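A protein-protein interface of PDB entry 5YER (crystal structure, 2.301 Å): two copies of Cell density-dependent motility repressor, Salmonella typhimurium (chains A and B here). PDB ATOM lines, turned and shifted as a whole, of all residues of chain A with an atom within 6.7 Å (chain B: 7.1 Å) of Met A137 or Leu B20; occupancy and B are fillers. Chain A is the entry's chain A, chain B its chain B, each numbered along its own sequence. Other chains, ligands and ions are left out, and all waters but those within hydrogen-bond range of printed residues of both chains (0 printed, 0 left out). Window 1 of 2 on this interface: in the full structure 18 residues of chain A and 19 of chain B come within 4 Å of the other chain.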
ATOM      1  N   HIS A  16      20.054  29.348   7.649  1.00  0.00           N
ATOM      2  CA  HIS A  16      20.418  28.650   8.880  1.00  0.00           C
ATOM      3  C   HIS A  16      19.220  28.498   9.812  1.00  0.00           C
ATOM      4  O   HIS A  16      19.009  27.429  10.395  1.00  0.00           O
ATOM      5  CB  HIS A  16      21.548  29.395   9.593  1.00  0.00           C
ATOM      6  CG  HIS A  16      22.865  29.337   8.883  1.00  0.00           C
ATOM      7  ND1 HIS A  16      23.456  28.150   8.504  1.00  0.00           N
ATOM      8  CD2 HIS A  16      23.711  30.320   8.494  1.00  0.00           C
ATOM      9  CE1 HIS A  16      24.607  28.406   7.906  1.00  0.00           C
ATOM     10  NE2 HIS A  16      24.785  29.715   7.887  1.00  0.00           N
ATOM     11  N   SER A  17      18.424  29.555   9.959  1.00  0.00           N
ATOM     12  CA  SER A  17      17.313  29.560  10.902  1.00  0.00           C
ATOM     13  C   SER A  17      16.094  28.792  10.409  1.00  0.00           C
ATOM     14  O   SER A  17      15.129  28.649  11.168  1.00  0.00           O
ATOM     15  CB  SER A  17      16.908  31.003  11.213  1.00  0.00           C
ATOM     16  OG  SER A  17      16.585  31.702  10.025  1.00  0.00           O
ATOM     17  N   LEU A  20      16.042  23.237   9.756  1.00  0.00           N
ATOM     18  CA  LEU A  20      15.565  22.150  10.606  1.00  0.00           C
ATOM     19  C   LEU A  20      14.052  22.180  10.786  1.00  0.00           C
ATOM     20  O   LEU A  20      13.431  21.128  10.974  1.00  0.00           O
ATOM     21  CB  LEU A  20      16.259  22.203  11.967  1.00  0.00           C
ATOM     22  CG  LEU A  20      15.968  21.031  12.908  1.00  0.00           C
ATOM     23  CD1 LEU A  20      16.368  19.717  12.258  1.00  0.00           C
ATOM     24  CD2 LEU A  20      16.673  21.209  14.244  1.00  0.00           C
ATOM     25  N   TYR A 107      20.153  36.472  16.997  1.00  0.00           N
ATOM     26  CA  TYR A 107      20.690  35.938  15.758  1.00  0.00           C
ATOM     27  C   TYR A 107      21.872  36.787  15.293  1.00  0.00           C
ATOM     28  O   TYR A 107      22.128  37.882  15.804  1.00  0.00           O
ATOM     29  CB  TYR A 107      19.611  35.889  14.678  1.00  0.00           C
ATOM     30  CG  TYR A 107      18.491  34.914  14.966  1.00  0.00           C
ATOM     31  CD1 TYR A 107      17.391  35.294  15.724  1.00  0.00           C
ATOM     32  CD2 TYR A 107      18.531  33.615  14.476  1.00  0.00           C
ATOM     33  CE1 TYR A 107      16.363  34.408  15.988  1.00  0.00           C
ATOM     34  CE2 TYR A 107      17.508  32.721  14.735  1.00  0.00           C
ATOM     35  CZ  TYR A 107      16.426  33.123  15.492  1.00  0.00           C
ATOM     36  OH  TYR A 107      15.404  32.239  15.754  1.00  0.00           O
ATOM     37  N   SER A 108      22.599  36.268  14.308  1.00  0.00           N
ATOM     38  CA  SER A 108      23.759  36.976  13.787  1.00  0.00           C
ATOM     39  C   SER A 108      23.340  38.296  13.145  1.00  0.00           C
ATOM     40  O   SER A 108      22.196  38.479  12.721  1.00  0.00           O
ATOM     41  CB  SER A 108      24.505  36.111  12.772  1.00  0.00           C
ATOM     42  OG  SER A 108      24.933  34.893  13.357  1.00  0.00           O
ATOM     43  N   PHE A 133      24.763  35.702  23.825  1.00  0.00           N
ATOM     44  CA  PHE A 133      24.941  34.585  22.907  1.00  0.00           C
ATOM     45  C   PHE A 133      24.384  34.965  21.544  1.00  0.00           C
ATOM     46  O   PHE A 133      23.267  35.483  21.452  1.00  0.00           O
ATOM     47  CB  PHE A 133      24.246  33.323  23.433  1.00  0.00           C
ATOM     48  CG  PHE A 133      24.670  32.061  22.740  1.00  0.00           C
ATOM     49  CD1 PHE A 133      24.036  31.642  21.582  1.00  0.00           C
ATOM     50  CD2 PHE A 133      25.701  31.288  23.250  1.00  0.00           C
ATOM     51  CE1 PHE A 133      24.424  30.481  20.942  1.00  0.00           C
ATOM     52  CE2 PHE A 133      26.094  30.124  22.615  1.00  0.00           C
ATOM     53  CZ  PHE A 133      25.454  29.720  21.460  1.00  0.00           C
ATOM     54  N   SER A 135      23.953  33.396  17.511  1.00  0.00           N
ATOM     55  CA  SER A 135      24.052  32.285  16.577  1.00  0.00           C
ATOM     56  C   SER A 135      22.943  32.415  15.544  1.00  0.00           C
ATOM     57  O   SER A 135      21.884  32.982  15.822  1.00  0.00           O
ATOM     58  CB  SER A 135      23.961  30.931  17.288  1.00  0.00           C
ATOM     59  OG  SER A 135      24.046  29.866  16.358  1.00  0.00           O
ATOM     60  N   SER A 136      23.200  31.882  14.351  1.00  0.00           N
ATOM     61  CA  SER A 136      22.224  31.913  13.269  1.00  0.00           C
ATOM     62  C   SER A 136      21.271  30.726  13.291  1.00  0.00           C
ATOM     63  O   SER A 136      20.292  30.724  12.536  1.00  0.00           O
ATOM     64  CB  SER A 136      22.937  31.965  11.913  1.00  0.00           C
ATOM     65  OG  SER A 136      23.489  33.247  11.677  1.00  0.00           O
ATOM     66  N   MET A 137      21.528  29.725  14.128  1.00  0.00           N
ATOM     67  CA  MET A 137      20.679  28.545  14.214  1.00  0.00           C
ATOM     68  C   MET A 137      19.576  28.796  15.234  1.00  0.00           C
ATOM     69  O   MET A 137      19.859  29.030  16.415  1.00  0.00           O
ATOM     70  CB  MET A 137      21.500  27.315  14.596  1.00  0.00           C
ATOM     71  CG  MET A 137      20.789  25.993  14.346  1.00  0.00           C
ATOM     72  SD  MET A 137      21.535  24.617  15.242  1.00  0.00           S
ATOM     73  CE  MET A 137      23.242  24.750  14.718  1.00  0.00           C
ATOM     74  N   SER A 138      18.322  28.754  14.775  1.00  0.00           N
ATOM     75  CA  SER A 138      17.194  28.947  15.681  1.00  0.00           C
ATOM     76  C   SER A 138      17.187  27.914  16.798  1.00  0.00           C
ATOM     77  O   SER A 138      16.767  28.216  17.921  1.00  0.00           O
ATOM     78  CB  SER A 138      15.880  28.886  14.905  1.00  0.00           C
ATOM     79  OG  SER A 138      15.736  30.011  14.058  1.00  0.00           O
ATOM     80  N   GLU A 139      17.650  26.694  16.515  1.00  0.00           N
ATOM     81  CA  GLU A 139      17.666  25.661  17.544  1.00  0.00           C
ATOM     82  C   GLU A 139      18.743  25.934  18.587  1.00  0.00           C
ATOM     83  O   GLU A 139      18.507  25.756  19.787  1.00  0.00           O
ATOM     84  CB  GLU A 139      17.862  24.290  16.899  1.00  0.00           C
ATOM     85  CG  GLU A 139      18.119  23.133  17.859  1.00  0.00           C
ATOM     86  CD  GLU A 139      16.999  22.877  18.847  1.00  0.00           C
ATOM     87  OE1 GLU A 139      16.957  23.540  19.904  1.00  0.00           O
ATOM     88  OE2 GLU A 139      16.160  21.996  18.566  1.00  0.00           O
ATOM     89  N   LEU A 140      19.928  26.375  18.154  1.00  0.00           N
ATOM     90  CA  LEU A 140      20.992  26.684  19.108  1.00  0.00           C
ATOM     91  C   LEU A 140      20.546  27.759  20.090  1.00  0.00           C
ATOM     92  O   LEU A 140      20.741  27.627  21.304  1.00  0.00           O
ATOM     93  CB  LEU A 140      22.264  27.118  18.378  1.00  0.00           C
ATOM     94  CG  LEU A 140      23.517  27.189  19.258  1.00  0.00           C
ATOM     95  CD1 LEU A 140      23.676  25.914  20.074  1.00  0.00           C
ATOM     96  CD2 LEU A 140      24.755  27.439  18.415  1.00  0.00           C
ATOM     97  N   LEU A 141      19.933  28.831  19.581  1.00  0.00           N
ATOM     98  CA  LEU A 141      19.393  29.860  20.463  1.00  0.00           C
ATOM     99  C   LEU A 141      18.262  29.318  21.325  1.00  0.00           C
ATOM    100  O   LEU A 141      18.096  29.747  22.473  1.00  0.00           O
ATOM    101  CB  LEU A 141      18.905  31.055  19.645  1.00  0.00           C
ATOM    102  CG  LEU A 141      19.951  31.834  18.846  1.00  0.00           C
ATOM    103  CD1 LEU A 141      19.287  32.918  18.010  1.00  0.00           C
ATOM    104  CD2 LEU A 141      20.995  32.432  19.774  1.00  0.00           C
ATOM    105  N   LYS A 142      17.474  28.382  20.791  1.00  0.00           N
ATOM    106  CA  LYS A 142      16.363  27.819  21.551  1.00  0.00           C
ATOM    107  C   LYS A 142      16.864  27.001  22.737  1.00  0.00           C
ATOM    108  O   LYS A 142      16.374  27.157  23.862  1.00  0.00           O
ATOM    109  CB  LYS A 142      15.487  26.961  20.638  1.00  0.00           C
ATOM    110  CG  LYS A 142      14.493  26.081  21.373  1.00  0.00           C
ATOM    111  CD  LYS A 142      13.658  25.264  20.402  1.00  0.00           C
ATOM    112  CE  LYS A 142      12.676  24.369  21.139  1.00  0.00           C
ATOM    113  NZ  LYS A 142      11.633  23.824  20.229  1.00  0.00           N
ATOM    114  N   GLN A 143      17.844  26.125  22.502  1.00  0.00           N
ATOM    115  CA  GLN A 143      18.358  25.282  23.577  1.00  0.00           C
ATOM    116  C   GLN A 143      19.017  26.114  24.670  1.00  0.00           C
ATOM    117  O   GLN A 143      18.847  25.832  25.862  1.00  0.00           O
ATOM    118  CB  GLN A 143      19.346  24.260  23.015  1.00  0.00           C
ATOM    119  CG  GLN A 143      19.725  23.162  23.993  1.00  0.00           C
ATOM    120  CD  GLN A 143      18.536  22.321  24.410  1.00  0.00           C
ATOM    121  OE1 GLN A 143      18.186  22.259  25.589  1.00  0.00           O
ATOM    122  NE2 GLN A 143      17.905  21.669  23.441  1.00  0.00           N
ATOM    123  N   LEU A 154      12.257  34.260  19.224  1.00  0.00           N
ATOM    124  CA  LEU A 154      12.210  32.987  18.526  1.00  0.00           C
ATOM    125  C   LEU A 154      10.905  32.851  17.757  1.00  0.00           C
ATOM    126  O   LEU A 154       9.882  33.417  18.155  1.00  0.00           O
ATOM    127  CB  LEU A 154      12.359  31.817  19.511  1.00  0.00           C
ATOM    128  CG  LEU A 154      13.725  31.716  20.195  1.00  0.00           C
ATOM    129  CD1 LEU A 154      13.694  30.697  21.325  1.00  0.00           C
ATOM    130  CD2 LEU A 154      14.810  31.372  19.185  1.00  0.00           C
ATOM    131  N   ALA B  14      32.208  26.630  14.659  1.00  0.00           N
ATOM    132  CA  ALA B  14      32.088  25.202  14.900  1.00  0.00           C
ATOM    133  C   ALA B  14      31.610  24.489  13.643  1.00  0.00           C
ATOM    134  O   ALA B  14      30.902  25.064  12.812  1.00  0.00           O
ATOM    135  CB  ALA B  14      31.124  24.917  16.056  1.00  0.00           C
ATOM    136  N   ALA B  15      32.014  23.227  13.513  1.00  0.00           N
ATOM    137  CA  ALA B  15      31.590  22.417  12.383  1.00  0.00           C
ATOM    138  C   ALA B  15      30.075  22.229  12.401  1.00  0.00           C
ATOM    139  O   ALA B  15      29.421  22.325  13.442  1.00  0.00           O
ATOM    140  CB  ALA B  15      32.294  21.060  12.403  1.00  0.00           C
ATOM    141  N   HIS B  16      29.520  21.957  11.217  1.00  0.00           N
ATOM    142  CA  HIS B  16      28.071  21.835  11.086  1.00  0.00           C
ATOM    143  C   HIS B  16      27.530  20.677  11.916  1.00  0.00           C
ATOM    144  O   HIS B  16      26.479  20.800  12.557  1.00  0.00           O
ATOM    145  CB  HIS B  16      27.691  21.659   9.615  1.00  0.00           C
ATOM    146  CG  HIS B  16      27.709  22.933   8.828  1.00  0.00           C
ATOM    147  ND1 HIS B  16      26.833  23.970   9.070  1.00  0.00           N
ATOM    148  CD2 HIS B  16      28.493  23.336   7.800  1.00  0.00           C
ATOM    149  CE1 HIS B  16      27.079  24.957   8.227  1.00  0.00           C
ATOM    150  NE2 HIS B  16      28.082  24.598   7.447  1.00  0.00           N
ATOM    151  N   SER B  17      28.234  19.549  11.924  1.00  0.00           N
ATOM    152  CA  SER B  17      27.780  18.347  12.612  1.00  0.00           C
ATOM    153  C   SER B  17      28.080  18.360  14.107  1.00  0.00           C
ATOM    154  O   SER B  17      27.835  17.353  14.778  1.00  0.00           O
ATOM    155  CB  SER B  17      28.414  17.109  11.971  1.00  0.00           C
ATOM    156  OG  SER B  17      29.806  17.294  11.769  1.00  0.00           O
ATOM    157  N   LEU B  18      28.588  19.471  14.643  1.00  0.00           N
ATOM    158  CA  LEU B  18      29.050  19.527  16.026  1.00  0.00           C
ATOM    159  C   LEU B  18      28.549  20.734  16.806  1.00  0.00           C
ATOM    160  O   LEU B  18      28.508  20.667  18.041  1.00  0.00           O
ATOM    161  CB  LEU B  18      30.588  19.521  16.064  1.00  0.00           C
ATOM    162  CG  LEU B  18      31.311  19.470  17.413  1.00  0.00           C
ATOM    163  CD1 LEU B  18      31.127  18.112  18.065  1.00  0.00           C
ATOM    164  CD2 LEU B  18      32.788  19.798  17.245  1.00  0.00           C
ATOM    165  N   SER B  19      28.146  21.817  16.137  1.00  0.00           N
ATOM    166  CA  SER B  19      27.872  23.073  16.831  1.00  0.00           C
ATOM    167  C   SER B  19      26.716  22.943  17.817  1.00  0.00           C
ATOM    168  O   SER B  19      26.790  23.461  18.936  1.00  0.00           O
ATOM    169  CB  SER B  19      27.587  24.174  15.809  1.00  0.00           C
ATOM    170  OG  SER B  19      27.324  25.414  16.442  1.00  0.00           O
ATOM    171  N   LEU B  20      25.644  22.251  17.436  1.00  0.00           N
ATOM    172  CA  LEU B  20      24.454  22.266  18.278  1.00  0.00           C
ATOM    173  C   LEU B  20      24.583  21.358  19.498  1.00  0.00           C
ATOM    174  O   LEU B  20      24.037  21.680  20.557  1.00  0.00           O
ATOM    175  CB  LEU B  20      23.225  21.882  17.458  1.00  0.00           C
ATOM    176  CG  LEU B  20      21.932  21.682  18.249  1.00  0.00           C
ATOM    177  CD1 LEU B  20      21.461  22.970  18.920  1.00  0.00           C
ATOM    178  CD2 LEU B  20      20.875  21.134  17.332  1.00  0.00           C
ATOM    179  N   GLY B  21      25.295  20.235  19.386  1.00  0.00           N
ATOM    180  CA  GLY B  21      25.425  19.340  20.524  1.00  0.00           C
ATOM    181  C   GLY B  21      26.491  19.751  21.519  1.00  0.00           C
ATOM    182  O   GLY B  21      26.438  19.346  22.684  1.00  0.00           O
ATOM    183  N   LEU B  22      27.457  20.561  21.091  1.00  0.00           N
ATOM    184  CA  LEU B  22      28.612  20.911  21.912  1.00  0.00           C
ATOM    185  C   LEU B  22      28.471  22.252  22.621  1.00  0.00           C
ATOM    186  O   LEU B  22      28.931  22.395  23.758  1.00  0.00           O
ATOM    187  CB  LEU B  22      29.878  20.921  21.048  1.00  0.00           C
ATOM    188  CG  LEU B  22      31.204  21.266  21.731  1.00  0.00           C
ATOM    189  CD1 LEU B  22      31.474  20.322  22.892  1.00  0.00           C
ATOM    190  CD2 LEU B  22      32.347  21.229  20.728  1.00  0.00           C
ATOM    191  N   LEU B  23      27.846  23.237  21.976  1.00  0.00           N
ATOM    192  CA  LEU B  23      27.771  24.575  22.557  1.00  0.00           C
ATOM    193  C   LEU B  23      26.962  24.653  23.849  1.00  0.00           C
ATOM    194  O   LEU B  23      27.420  25.338  24.781  1.00  0.00           O
ATOM    195  CB  LEU B  23      27.213  25.558  21.519  1.00  0.00           C
ATOM    196  CG  LEU B  23      28.236  26.432  20.788  1.00  0.00           C
ATOM    197  CD1 LEU B  23      29.040  27.265  21.775  1.00  0.00           C
ATOM    198  CD2 LEU B  23      29.154  25.580  19.925  1.00  0.00           C
ATOM    199  N   PRO B  24      25.782  24.029  23.980  1.00  0.00           N
ATOM    200  CA  PRO B  24      25.012  24.209  25.226  1.00  0.00           C
ATOM    201  C   PRO B  24      25.754  23.780  26.481  1.00  0.00           C
ATOM    202  O   PRO B  24      25.743  24.513  27.478  1.00  0.00           O
ATOM    203  CB  PRO B  24      23.759  23.358  24.979  1.00  0.00           C
ATOM    204  CG  PRO B  24      23.605  23.357  23.509  1.00  0.00           C
ATOM    205  CD  PRO B  24      25.002  23.284  22.975  1.00  0.00           C
ATOM    206  N   THR B  25      26.402  22.612  26.466  1.00  0.00           N
ATOM    207  CA  THR B  25      27.099  22.156  27.666  1.00  0.00           C
ATOM    208  C   THR B  25      28.318  23.018  27.971  1.00  0.00           C
ATOM    209  O   THR B  25      28.727  23.119  29.133  1.00  0.00           O
ATOM    210  CB  THR B  25      27.507  20.688  27.527  1.00  0.00           C
ATOM    211  OG1 THR B  25      28.124  20.246  28.743  1.00  0.00           O
ATOM    212  CG2 THR B  25      28.482  20.499  26.372  1.00  0.00           C
ATOM    213  N   VAL B  38      28.886  32.462  17.831  1.00  0.00           N
ATOM    214  CA  VAL B  38      29.084  31.168  17.189  1.00  0.00           C
ATOM    215  C   VAL B  38      28.478  31.207  15.794  1.00  0.00           C
ATOM    216  O   VAL B  38      27.378  31.736  15.597  1.00  0.00           O
ATOM    217  CB  VAL B  38      28.463  30.029  18.021  1.00  0.00           C
ATOM    218  CG1 VAL B  38      28.909  28.672  17.491  1.00  0.00           C
ATOM    219  CG2 VAL B  38      28.826  30.187  19.490  1.00  0.00           C
ATOM    220  N   ALA B  40      28.209  28.408  12.315  1.00  0.00           N
ATOM    221  CA  ALA B  40      28.513  27.094  11.769  1.00  0.00           C
ATOM    222  C   ALA B  40      29.300  27.226  10.473  1.00  0.00           C
ATOM    223  O   ALA B  40      29.011  28.087   9.637  1.00  0.00           O
ATOM    224  CB  ALA B  40      27.229  26.304  11.528  1.00  0.00           C
ATOM    225  N   MET B 137      24.137  18.999   8.557  1.00  0.00           N
ATOM    226  CA  MET B 137      23.531  19.283   9.852  1.00  0.00           C
ATOM    227  C   MET B 137      23.076  17.969  10.475  1.00  0.00           C
ATOM    228  O   MET B 137      22.201  17.288   9.929  1.00  0.00           O
ATOM    229  CB  MET B 137      22.360  20.250   9.698  1.00  0.00           C
ATOM    230  CG  MET B 137      21.863  20.832  11.013  1.00  0.00           C
ATOM    231  SD  MET B 137      20.457  21.942  10.801  1.00  0.00           S
ATOM    232  CE  MET B 137      21.021  22.950   9.433  1.00  0.00           C
ATOM    233  N   SER B 138      23.679  17.609  11.612  1.00  0.00           N
ATOM    234  CA  SER B 138      23.407  16.309  12.219  1.00  0.00           C
ATOM    235  C   SER B 138      21.939  16.164  12.595  1.00  0.00           C
ATOM    236  O   SER B 138      21.343  15.097  12.400  1.00  0.00           O
ATOM    237  CB  SER B 138      24.295  16.111  13.448  1.00  0.00           C
ATOM    238  OG  SER B 138      25.618  15.774  13.072  1.00  0.00           O
ATOM    239  N   GLU B 139      21.334  17.225  13.125  1.00  0.00           N
ATOM    240  CA  GLU B 139      19.960  17.134  13.598  1.00  0.00           C
ATOM    241  C   GLU B 139      18.942  17.178  12.469  1.00  0.00           C
ATOM    242  O   GLU B 139      17.786  16.795  12.681  1.00  0.00           O
ATOM    243  CB  GLU B 139      19.679  18.250  14.605  1.00  0.00           C
ATOM    244  CG  GLU B 139      20.256  17.974  15.983  1.00  0.00           C
ATOM    245  CD  GLU B 139      21.771  18.082  16.013  1.00  0.00           C
ATOM    246  OE1 GLU B 139      22.320  18.944  15.294  1.00  0.00           O
ATOM    247  OE2 GLU B 139      22.412  17.306  16.753  1.00  0.00           O
ATOM    248  N   TYR B 157      25.872  11.003  20.794  1.00  0.00           N
ATOM    249  CA  TYR B 157      25.382  12.053  21.682  1.00  0.00           C
ATOM    250  C   TYR B 157      24.111  12.714  21.164  1.00  0.00           C
ATOM    251  O   TYR B 157      23.369  13.304  21.956  1.00  0.00           O
ATOM    252  CB  TYR B 157      26.465  13.113  21.909  1.00  0.00           C
ATOM    253  CG  TYR B 157      26.899  13.868  20.668  1.00  0.00           C
ATOM    254  CD1 TYR B 157      26.174  14.958  20.198  1.00  0.00           C
ATOM    255  CD2 TYR B 157      28.047  13.500  19.978  1.00  0.00           C
ATOM    256  CE1 TYR B 157      26.573  15.649  19.069  1.00  0.00           C
ATOM    257  CE2 TYR B 157      28.455  14.189  18.851  1.00  0.00           C
ATOM    258  CZ  TYR B 157      27.713  15.260  18.400  1.00  0.00           C
ATOM    259  OH  TYR B 157      28.113  15.949  17.277  1.00  0.00           O
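The side-chain hydroxyl of Ser A135 lies close to the backbone NH of Met A137 (3.4 Å).
SD of Met A137 sits at hydrogen-bond distance from N of Leu A140 (3.8 Å).
Of the 16 printed residues of chain A, 7 touch a printed residue of chain B.
Of the 18 printed residues of chain B, 6 touch a printed residue of chain A.
Printed residues of chain B that touch a printed residue of chain A: Ser B19, Leu B20, Leu B23, Pro B24, Val B38 and Glu B139.
Hydrophobic or aromatic side chains of chain B that line the printed part of chain A: Leu B20, Leu B23, Pro B24 and Val B38.
Of chain B, only Leu B20 comes within 4 Å of Met A137.
Of chain A, only Met A137, Glu A139 and Leu A140 come within 4 Å of Leu B20.
Of the printed residues of chain B, Glu A139 touches Leu B20.
Printed residues of chain B within 4 Å of Leu A140: Ser B19, Leu B20 and Leu B23.
The nearest residue of chain B that does not touch Met A137 is Ser B19 (4.5 Å).
Among the printed residues, merely in contact across the chains: Leu A20 with Glu B139, Phe A133 with Val B38, Ser A135 with Val B38, Met A137 with Leu B20, Glu A139 with Leu B20, Leu A140 with Ser B19, Leu A140 with Leu B20, Leu A140 with Leu B23 and Gln A143 with Pro B24.
Leu A20 touches Glu B139, and with the chains exchanged Glu A139 touches Leu B20.
Met A137 touches Leu B20, but with the chains exchanged Leu A20 does not touch Met B137 (4.4 Å).
Of the 9 pairs that touch across the chains among the printed residues, 2 have their exchanged pair printed and touching as well.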
